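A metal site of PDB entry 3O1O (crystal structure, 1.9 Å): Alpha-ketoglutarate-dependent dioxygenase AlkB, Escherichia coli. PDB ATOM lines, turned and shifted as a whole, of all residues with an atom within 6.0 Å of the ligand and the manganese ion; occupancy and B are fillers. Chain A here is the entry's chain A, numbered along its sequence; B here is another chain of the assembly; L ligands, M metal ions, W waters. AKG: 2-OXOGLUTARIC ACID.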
ATOM      1  N   MET A  51       5.738  14.009  21.106  1.00  0.00           N
ATOM      2  CA  MET A  51       6.960  13.229  21.340  1.00  0.00           C
ATOM      3  C   MET A  51       7.974  13.895  22.273  1.00  0.00           C
ATOM      4  O   MET A  51       7.990  15.123  22.460  1.00  0.00           O
ATOM      5  CB  MET A  51       7.661  12.953  20.008  1.00  0.00           C
ATOM      6  CG  MET A  51       6.825  12.123  19.066  1.00  0.00           C
ATOM      7  SD  MET A  51       7.586  11.953  17.431  1.00  0.00           S
ATOM      8  CE  MET A  51       6.663  10.504  16.862  1.00  0.00           C
ATOM      9  N   LEU A 108      12.565   6.909  22.047  1.00  0.00           N
ATOM     10  CA  LEU A 108      11.554   7.876  21.592  1.00  0.00           C
ATOM     11  C   LEU A 108      10.282   7.609  22.387  1.00  0.00           C
ATOM     12  O   LEU A 108       9.792   6.478  22.404  1.00  0.00           O
ATOM     13  CB  LEU A 108      11.278   7.712  20.098  1.00  0.00           C
ATOM     14  CG  LEU A 108      10.131   8.523  19.482  1.00  0.00           C
ATOM     15  CD1 LEU A 108      10.305  10.030  19.732  1.00  0.00           C
ATOM     16  CD2 LEU A 108      10.025   8.226  17.991  1.00  0.00           C
ATOM     17  N   ASN A 110       6.401   8.385  22.745  1.00  0.00           N
ATOM     18  CA  ASN A 110       5.220   8.864  22.003  1.00  0.00           C
ATOM     19  C   ASN A 110       3.992   8.939  22.903  1.00  0.00           C
ATOM     20  O   ASN A 110       3.703   7.978  23.617  1.00  0.00           O
ATOM     21  CB  ASN A 110       4.886   7.929  20.851  1.00  0.00           C
ATOM     22  CG  ASN A 110       5.987   7.820  19.814  1.00  0.00           C
ATOM     23  OD1 ASN A 110       6.274   6.737  19.291  1.00  0.00           O
ATOM     24  ND2 ASN A 110       6.644   8.915  19.546  1.00  0.00           N
ATOM     25  N   TYR A 112      -0.139   9.508  22.733  1.00  0.00           N
ATOM     26  CA  TYR A 112      -1.300   9.520  21.844  1.00  0.00           C
ATOM     27  C   TYR A 112      -2.534   9.970  22.575  1.00  0.00           C
ATOM     28  O   TYR A 112      -3.000   9.270  23.471  1.00  0.00           O
ATOM     29  CB  TYR A 112      -1.606   8.116  21.330  1.00  0.00           C
ATOM     30  CG  TYR A 112      -0.548   7.532  20.436  1.00  0.00           C
ATOM     31  CD1 TYR A 112       0.626   7.036  20.972  1.00  0.00           C
ATOM     32  CD2 TYR A 112      -0.736   7.467  19.069  1.00  0.00           C
ATOM     33  CE1 TYR A 112       1.609   6.486  20.158  1.00  0.00           C
ATOM     34  CE2 TYR A 112       0.229   6.935  18.241  1.00  0.00           C
ATOM     35  CZ  TYR A 112       1.394   6.443  18.794  1.00  0.00           C
ATOM     36  OH  TYR A 112       2.348   5.920  17.970  1.00  0.00           O
ATOM     37  N   LEU A 118      -0.040   7.210  13.677  1.00  0.00           N
ATOM     38  CA  LEU A 118       1.256   7.246  13.051  1.00  0.00           C
ATOM     39  C   LEU A 118       1.124   6.449  11.753  1.00  0.00           C
ATOM     40  O   LEU A 118       1.036   5.214  11.760  1.00  0.00           O
ATOM     41  CB  LEU A 118       2.311   6.635  13.976  1.00  0.00           C
ATOM     42  CG  LEU A 118       3.724   7.242  14.014  1.00  0.00           C
ATOM     43  CD1 LEU A 118       3.665   8.765  14.187  1.00  0.00           C
ATOM     44  CD2 LEU A 118       4.590   6.604  15.135  1.00  0.00           C
ATOM     45  N   HIS A 121       5.099   3.527   8.259  1.00  0.00           N
ATOM     46  CA  HIS A 121       6.463   3.971   8.012  1.00  0.00           C
ATOM     47  C   HIS A 121       7.433   2.849   8.355  1.00  0.00           C
ATOM     48  O   HIS A 121       7.047   1.840   8.938  1.00  0.00           O
ATOM     49  CB  HIS A 121       6.805   5.224   8.831  1.00  0.00           C
ATOM     50  CG  HIS A 121       6.806   4.975  10.301  1.00  0.00           C
ATOM     51  ND1 HIS A 121       5.652   4.964  11.052  1.00  0.00           N
ATOM     52  CD2 HIS A 121       7.811   4.700  11.169  1.00  0.00           C
ATOM     53  CE1 HIS A 121       5.948   4.693  12.311  1.00  0.00           C
ATOM     54  NE2 HIS A 121       7.251   4.540  12.409  1.00  0.00           N
ATOM     55  N   GLN A 122       8.689   3.061   8.001  1.00  0.00           N
ATOM     56  CA  GLN A 122       9.746   2.108   8.328  1.00  0.00           C
ATOM     57  C   GLN A 122      10.744   2.795   9.225  1.00  0.00           C
ATOM     58  O   GLN A 122      11.029   3.970   9.023  1.00  0.00           O
ATOM     59  CB  GLN A 122      10.498   1.690   7.078  1.00  0.00           C
ATOM     60  CG  GLN A 122       9.721   0.984   6.012  1.00  0.00           C
ATOM     61  CD  GLN A 122      10.566   0.777   4.773  1.00  0.00           C
ATOM     62  OE1 GLN A 122      10.902   1.737   4.060  1.00  0.00           O
ATOM     63  NE2 GLN A 122      10.948  -0.473   4.521  1.00  0.00           N
ATOM     64  N   ASP A 123      11.269   2.067  10.202  1.00  0.00           N
ATOM     65  CA  ASP A 123      12.405   2.546  10.953  1.00  0.00           C
ATOM     66  C   ASP A 123      13.633   2.096  10.186  1.00  0.00           C
ATOM     67  O   ASP A 123      13.939   0.918  10.154  1.00  0.00           O
ATOM     68  CB  ASP A 123      12.420   1.964  12.358  1.00  0.00           C
ATOM     69  CG  ASP A 123      11.422   2.611  13.279  1.00  0.00           C
ATOM     70  OD1 ASP A 123      10.342   3.040  12.808  1.00  0.00           O
ATOM     71  OD2 ASP A 123      11.722   2.683  14.485  1.00  0.00           O
ATOM     72  N   SER A 135       9.512  -1.971  21.368  1.00  0.00           N
ATOM     73  CA  SER A 135       8.412  -1.005  21.395  1.00  0.00           C
ATOM     74  C   SER A 135       7.425  -1.383  22.500  1.00  0.00           C
ATOM     75  O   SER A 135       6.755  -2.418  22.414  1.00  0.00           O
ATOM     76  CB  SER A 135       7.718  -1.007  20.015  1.00  0.00           C
ATOM     77  OG  SER A 135       6.733   0.032  19.924  1.00  0.00           O
ATOM     78  N   SER A 137       4.075  -0.595  24.966  1.00  0.00           N
ATOM     79  CA  SER A 137       2.788   0.099  24.959  1.00  0.00           C
ATOM     80  C   SER A 137       2.330   0.310  26.374  1.00  0.00           C
ATOM     81  O   SER A 137       2.425  -0.614  27.185  1.00  0.00           O
ATOM     82  CB  SER A 137       1.688  -0.726  24.248  1.00  0.00           C
ATOM     83  OG  SER A 137       1.964  -0.858  22.882  1.00  0.00           O
ATOM     84  N   PHE A 144      -2.186  -1.643  16.088  1.00  0.00           N
ATOM     85  CA  PHE A 144      -0.861  -1.600  15.498  1.00  0.00           C
ATOM     86  C   PHE A 144      -0.923  -2.318  14.172  1.00  0.00           C
ATOM     87  O   PHE A 144      -1.479  -3.426  14.093  1.00  0.00           O
ATOM     88  CB  PHE A 144       0.110  -2.271  16.474  1.00  0.00           C
ATOM     89  CG  PHE A 144       1.535  -2.326  16.004  1.00  0.00           C
ATOM     90  CD1 PHE A 144       2.293  -1.166  15.842  1.00  0.00           C
ATOM     91  CD2 PHE A 144       2.151  -3.558  15.788  1.00  0.00           C
ATOM     92  CE1 PHE A 144       3.602  -1.228  15.430  1.00  0.00           C
ATOM     93  CE2 PHE A 144       3.469  -3.631  15.394  1.00  0.00           C
ATOM     94  CZ  PHE A 144       4.199  -2.454  15.203  1.00  0.00           C
ATOM     95  N   LEU A 160      -2.770  -3.580  20.604  1.00  0.00           N
ATOM     96  CA  LEU A 160      -1.686  -3.520  21.585  1.00  0.00           C
ATOM     97  C   LEU A 160      -2.300  -2.915  22.841  1.00  0.00           C
ATOM     98  O   LEU A 160      -2.895  -1.834  22.804  1.00  0.00           O
ATOM     99  CB  LEU A 160      -0.524  -2.664  21.093  1.00  0.00           C
ATOM    100  CG  LEU A 160       0.191  -3.180  19.823  1.00  0.00           C
ATOM    101  CD1 LEU A 160       1.430  -2.342  19.547  1.00  0.00           C
ATOM    102  CD2 LEU A 160       0.608  -4.629  20.048  1.00  0.00           C
ATOM    103  N   TRP A 168      10.924  -6.166  16.890  1.00  0.00           N
ATOM    104  CA  TRP A 168      11.227  -6.647  15.549  1.00  0.00           C
ATOM    105  C   TRP A 168      12.682  -6.390  15.184  1.00  0.00           C
ATOM    106  O   TRP A 168      13.303  -5.432  15.641  1.00  0.00           O
ATOM    107  CB  TRP A 168      10.221  -6.134  14.511  1.00  0.00           C
ATOM    108  CG  TRP A 168      10.075  -4.631  14.321  1.00  0.00           C
ATOM    109  CD1 TRP A 168      10.621  -3.884  13.318  1.00  0.00           C
ATOM    110  CD2 TRP A 168       9.267  -3.729  15.099  1.00  0.00           C
ATOM    111  NE1 TRP A 168      10.222  -2.577  13.434  1.00  0.00           N
ATOM    112  CE2 TRP A 168       9.404  -2.454  14.522  1.00  0.00           C
ATOM    113  CE3 TRP A 168       8.476  -3.880  16.230  1.00  0.00           C
ATOM    114  CZ2 TRP A 168       8.762  -1.331  15.036  1.00  0.00           C
ATOM    115  CZ3 TRP A 168       7.836  -2.761  16.757  1.00  0.00           C
ATOM    116  CH2 TRP A 168       7.979  -1.499  16.153  1.00  0.00           C
ATOM    117  N   HIS A 177       5.114  -0.327   9.470  1.00  0.00           N
ATOM    118  CA  HIS A 177       4.269  -0.491  10.633  1.00  0.00           C
ATOM    119  C   HIS A 177       3.674   0.876  10.944  1.00  0.00           C
ATOM    120  O   HIS A 177       4.143   1.903  10.446  1.00  0.00           O
ATOM    121  CB  HIS A 177       5.104  -0.997  11.823  1.00  0.00           C
ATOM    122  CG  HIS A 177       6.254  -0.095  12.163  1.00  0.00           C
ATOM    123  ND1 HIS A 177       7.457  -0.128  11.482  1.00  0.00           N
ATOM    124  CD2 HIS A 177       6.371   0.889  13.089  1.00  0.00           C
ATOM    125  CE1 HIS A 177       8.269   0.775  11.993  1.00  0.00           C
ATOM    126  NE2 HIS A 177       7.639   1.417  12.956  1.00  0.00           N
ATOM    127  N   GLY A 178       2.668   0.925  11.815  1.00  0.00           N
ATOM    128  CA  GLY A 178       2.000   2.173  12.103  1.00  0.00           C
ATOM    129  C   GLY A 178       0.950   1.954  13.162  1.00  0.00           C
ATOM    130  O   GLY A 178       0.726   0.819  13.616  1.00  0.00           O
ATOM    131  N   ILE A 179       0.338   3.046  13.572  1.00  0.00           N
ATOM    132  CA  ILE A 179      -0.721   3.046  14.577  1.00  0.00           C
ATOM    133  C   ILE A 179      -1.972   3.738  14.002  1.00  0.00           C
ATOM    134  O   ILE A 179      -1.894   4.852  13.478  1.00  0.00           O
ATOM    135  CB  ILE A 179      -0.263   3.754  15.856  1.00  0.00           C
ATOM    136  CG1 ILE A 179       0.889   2.958  16.506  1.00  0.00           C
ATOM    137  CG2 ILE A 179      -1.433   3.906  16.849  1.00  0.00           C
ATOM    138  CD1 ILE A 179       0.447   1.720  17.262  1.00  0.00           C
ATOM    139  N   ARG A 194      -2.482   7.069  25.424  1.00  0.00           N
ATOM    140  CA  ARG A 194      -1.564   5.964  25.277  1.00  0.00           C
ATOM    141  C   ARG A 194      -0.135   6.516  25.199  1.00  0.00           C
ATOM    142  O   ARG A 194       0.107   7.549  24.582  1.00  0.00           O
ATOM    143  CB  ARG A 194      -1.890   5.169  24.005  1.00  0.00           C
ATOM    144  CG  ARG A 194      -0.838   4.115  23.640  1.00  0.00           C
ATOM    145  CD  ARG A 194      -1.212   3.341  22.396  1.00  0.00           C
ATOM    146  NE  ARG A 194      -0.287   2.240  22.138  1.00  0.00           N
ATOM    147  CZ  ARG A 194       0.734   2.305  21.294  1.00  0.00           C
ATOM    148  NH1 ARG A 194       0.964   3.417  20.607  1.00  0.00           N
ATOM    149  NH2 ARG A 194       1.527   1.246  21.119  1.00  0.00           N
ATOM    150  N   ASN A 196       3.892   5.185  24.169  1.00  0.00           N
ATOM    151  CA  ASN A 196       4.744   4.126  23.634  1.00  0.00           C
ATOM    152  C   ASN A 196       6.210   4.507  23.832  1.00  0.00           C
ATOM    153  O   ASN A 196       6.581   5.687  23.696  1.00  0.00           O
ATOM    154  CB  ASN A 196       4.423   3.903  22.165  1.00  0.00           C
ATOM    155  CG  ASN A 196       5.512   3.123  21.436  1.00  0.00           C
ATOM    156  OD1 ASN A 196       6.477   3.704  20.962  1.00  0.00           O
ATOM    157  ND2 ASN A 196       5.346   1.820  21.326  1.00  0.00           N
ATOM    158  N   THR A 198       9.819   3.626  22.381  1.00  0.00           N
ATOM    159  CA  THR A 198      10.531   2.965  21.304  1.00  0.00           C
ATOM    160  C   THR A 198      12.053   3.052  21.460  1.00  0.00           C
ATOM    161  O   THR A 198      12.627   4.147  21.345  1.00  0.00           O
ATOM    162  CB  THR A 198      10.102   3.530  19.955  1.00  0.00           C
ATOM    163  OG1 THR A 198       8.705   3.236  19.761  1.00  0.00           O
ATOM    164  CG2 THR A 198      10.919   2.897  18.821  1.00  0.00           C
ATOM    165  N   ARG A 200      15.941   2.136  20.426  1.00  0.00           N
ATOM    166  CA  ARG A 200      16.714   1.819  19.243  1.00  0.00           C
ATOM    167  C   ARG A 200      18.198   1.923  19.536  1.00  0.00           C
ATOM    168  O   ARG A 200      18.611   2.581  20.483  1.00  0.00           O
ATOM    169  CB  ARG A 200      16.369   2.789  18.097  1.00  0.00           C
ATOM    170  CG  ARG A 200      14.894   2.821  17.696  1.00  0.00           C
ATOM    171  CD  ARG A 200      14.654   3.947  16.707  1.00  0.00           C
ATOM    172  NE  ARG A 200      13.283   4.032  16.199  1.00  0.00           N
ATOM    173  CZ  ARG A 200      12.356   4.879  16.652  1.00  0.00           C
ATOM    174  NH1 ARG A 200      12.638   5.721  17.638  1.00  0.00           N
ATOM    175  NH2 ARG A 200      11.156   4.880  16.102  1.00  0.00           N
ATOM    176  P   MFT B   8       7.138   8.718   6.470  1.00  0.00           P
ATOM    177  N1  MFT B   8       7.540   8.849  11.412  1.00  0.00           N
ATOM    178  C2  MFT B   8       7.978   8.655  12.738  1.00  0.00           C
ATOM    179  O2  MFT B   8       7.270   9.045  13.697  1.00  0.00           O
ATOM    180  N3  MFT B   8       9.165   8.061  12.993  1.00  0.00           N
ATOM    181  C4  MFT B   8       9.927   7.637  11.979  1.00  0.00           C
ATOM    182  O4  MFT B   8      11.016   7.070  12.187  1.00  0.00           O
ATOM    183  C5  MFT B   8       9.484   7.809  10.586  1.00  0.00           C
ATOM    184  C6  MFT B   8       8.268   8.419  10.370  1.00  0.00           C
ATOM    185  C1' MFT B   8       6.220   9.434  11.172  1.00  0.00           C
ATOM    186  O1P MFT B   8       8.489   9.363   6.709  1.00  0.00           O
ATOM    187  C2' MFT B   8       6.142  10.684  10.329  1.00  0.00           C
ATOM    188  C21 MFT B   8       9.629   7.886  14.374  1.00  0.00           C
ATOM    189  O2P MFT B   8       7.053   7.235   6.375  1.00  0.00           O
ATOM    190  C3' MFT B   8       4.767  10.542   9.710  1.00  0.00           C
ATOM    191  O3' MFT B   8       3.880  10.919  10.762  1.00  0.00           O
ATOM    192  C4' MFT B   8       4.615   9.053   9.478  1.00  0.00           C
ATOM    193  O4' MFT B   8       5.487   8.445  10.435  1.00  0.00           O
ATOM    194  C5' MFT B   8       4.987   8.621   8.070  1.00  0.00           C
ATOM    195  O5' MFT B   8       6.206   9.246   7.682  1.00  0.00           O
ATOM    196  C5M MFT B   8      10.362   7.322   9.462  1.00  0.00           C
HETATM  197  C1  AKG L   1       7.772   4.758  16.405  1.00  0.00           C
HETATM  198  O1  AKG L   1       7.886   5.451  17.454  1.00  0.00           O
HETATM  199  O2  AKG L   1       8.595   4.803  15.453  1.00  0.00           O
HETATM  200  C2  AKG L   1       6.591   3.893  16.328  1.00  0.00           C
HETATM  201  O5  AKG L   1       6.411   3.202  15.348  1.00  0.00           O
HETATM  202  C3  AKG L   1       5.605   3.893  17.472  1.00  0.00           C
HETATM  203  C4  AKG L   1       4.720   2.657  17.379  1.00  0.00           C
HETATM  204  C5  AKG L   1       3.740   2.610  18.538  1.00  0.00           C
HETATM  205  O3  AKG L   1       3.391   3.690  19.075  1.00  0.00           O
HETATM  206  O4  AKG L   1       3.322   1.495  18.933  1.00  0.00           O
HETATM  207 MN    MN M   1       8.262   3.265  13.866  1.00  0.00          MN
HETATM  208  O   HOH W   1       8.041   1.584  17.729  1.00  0.00           O
HETATM  209  O   HOH W   2       4.624  -1.029  18.689  1.00  0.00           O
HETATM  210  O   HOH W   3       9.452   1.911  15.409  1.00  0.00           O
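The guanidinium group (NH2) of Arg 200 is in salt-bridge range of an oxygen (O1) of the ligand, at 3.6 Å.
An oxygen (O3) of the ligand is in hydrogen-bond range of the side-chain hydroxyl of Tyr 112, at 2.7 Å.
The side-chain amide oxygen (OD1) of Asn 110 lies close to an oxygen (O1) of the ligand, 2.8 Å away.
An oxygen (O4) of the ligand lies within salt-bridge range of the guanidinium group (NH2) of Arg 194 (2.8 Å).
An oxygen (O4) of the ligand sits at hydrogen-bond distance from the side-chain amide nitrogen (ND2) of Asn 196.
The side-chain hydroxyl (OG1) of Thr 198 sits at hydrogen-bond distance from an oxygen (O1) of the ligand (3.3 Å).
NE of Arg 200 lies within salt-bridge range of OD2 of Asp 123, 2.7 Å away.
The backbone carbonyl oxygen of Arg 194 is in hydrogen-bond range of the backbone NH of Tyr 112, 2.7 Å away.
The backbone NH (N) of Asn 196 lies within hydrogen-bond range of the backbone carbonyl oxygen (O) of Asn 110 (2.9 Å).
The guanidinium group (NH2) of Arg 194 lies within hydrogen-bond range of the side-chain hydroxyl (OG) of Ser 137.
OD1 of Asn 196 lies within hydrogen-bond range of OG1 of Thr 198.
The side-chain hydroxyl of Ser 135 is in hydrogen-bond range of the side-chain amide nitrogen of Asn 196, 2.7 Å away.
The backbone carbonyl oxygen (O) of Thr 198 sits at hydrogen-bond distance from the backbone NH (N) of Leu 108 (2.9 Å).
The backbone NH of Ile 179 is in hydrogen-bond range of the backbone carbonyl oxygen of Leu 118.
Leu 108 touches the ligand.
CD2 of Leu 118 touches C2 of the ligand (3.6 Å).
OG of Ser 135 touches O4 of the ligand (3.8 Å).
Ile 179 touches the ligand.
MFT 8 of chain B touches the ligand (C21 to O2, 3.4 Å).
Hydrophobic or aromatic side chains that line the ligand: Leu 108, Tyr 112, Leu 118, His 121, His 177 and Ile 179.
Within 4 Å of the ligand: Leu 108, Asn 110, Tyr 112, Leu 118, His 121, Asp 123, Ser 135, His 177, Ile 179, Arg 194, Asn 196, Thr 198, Arg 200 and MFT 8 of chain B.
Merely in contact with the manganese ion: Arg 200 (3.998 Å).
Within 4 Å of the manganese ion: His 121, Asp 123, His 177 and Arg 200.
The manganese ion is bound by NE2 of His 177 (2.2 Å), NE2 of His 121 (2.2 Å), O2 of the ligand (2.2 Å), OD1 of Asp 123 (2.3 Å), water W3 (2.4 Å) and O5 of the ligand (2.4 Å).
The manganese ion has six donor atoms within binding distance.
Water W3 lies within hydrogen-bond range of the side-chain carboxylate of Asp 123 and the guanidinium group of Arg 200.
Water W2 bridges OG of Ser 135 and O4 of the ligand.
Water W1 bridges the side-chain hydroxyl of Thr 198 (2.7 Å) and the side-chain hydroxyl of Ser 135 (3.0 Å).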
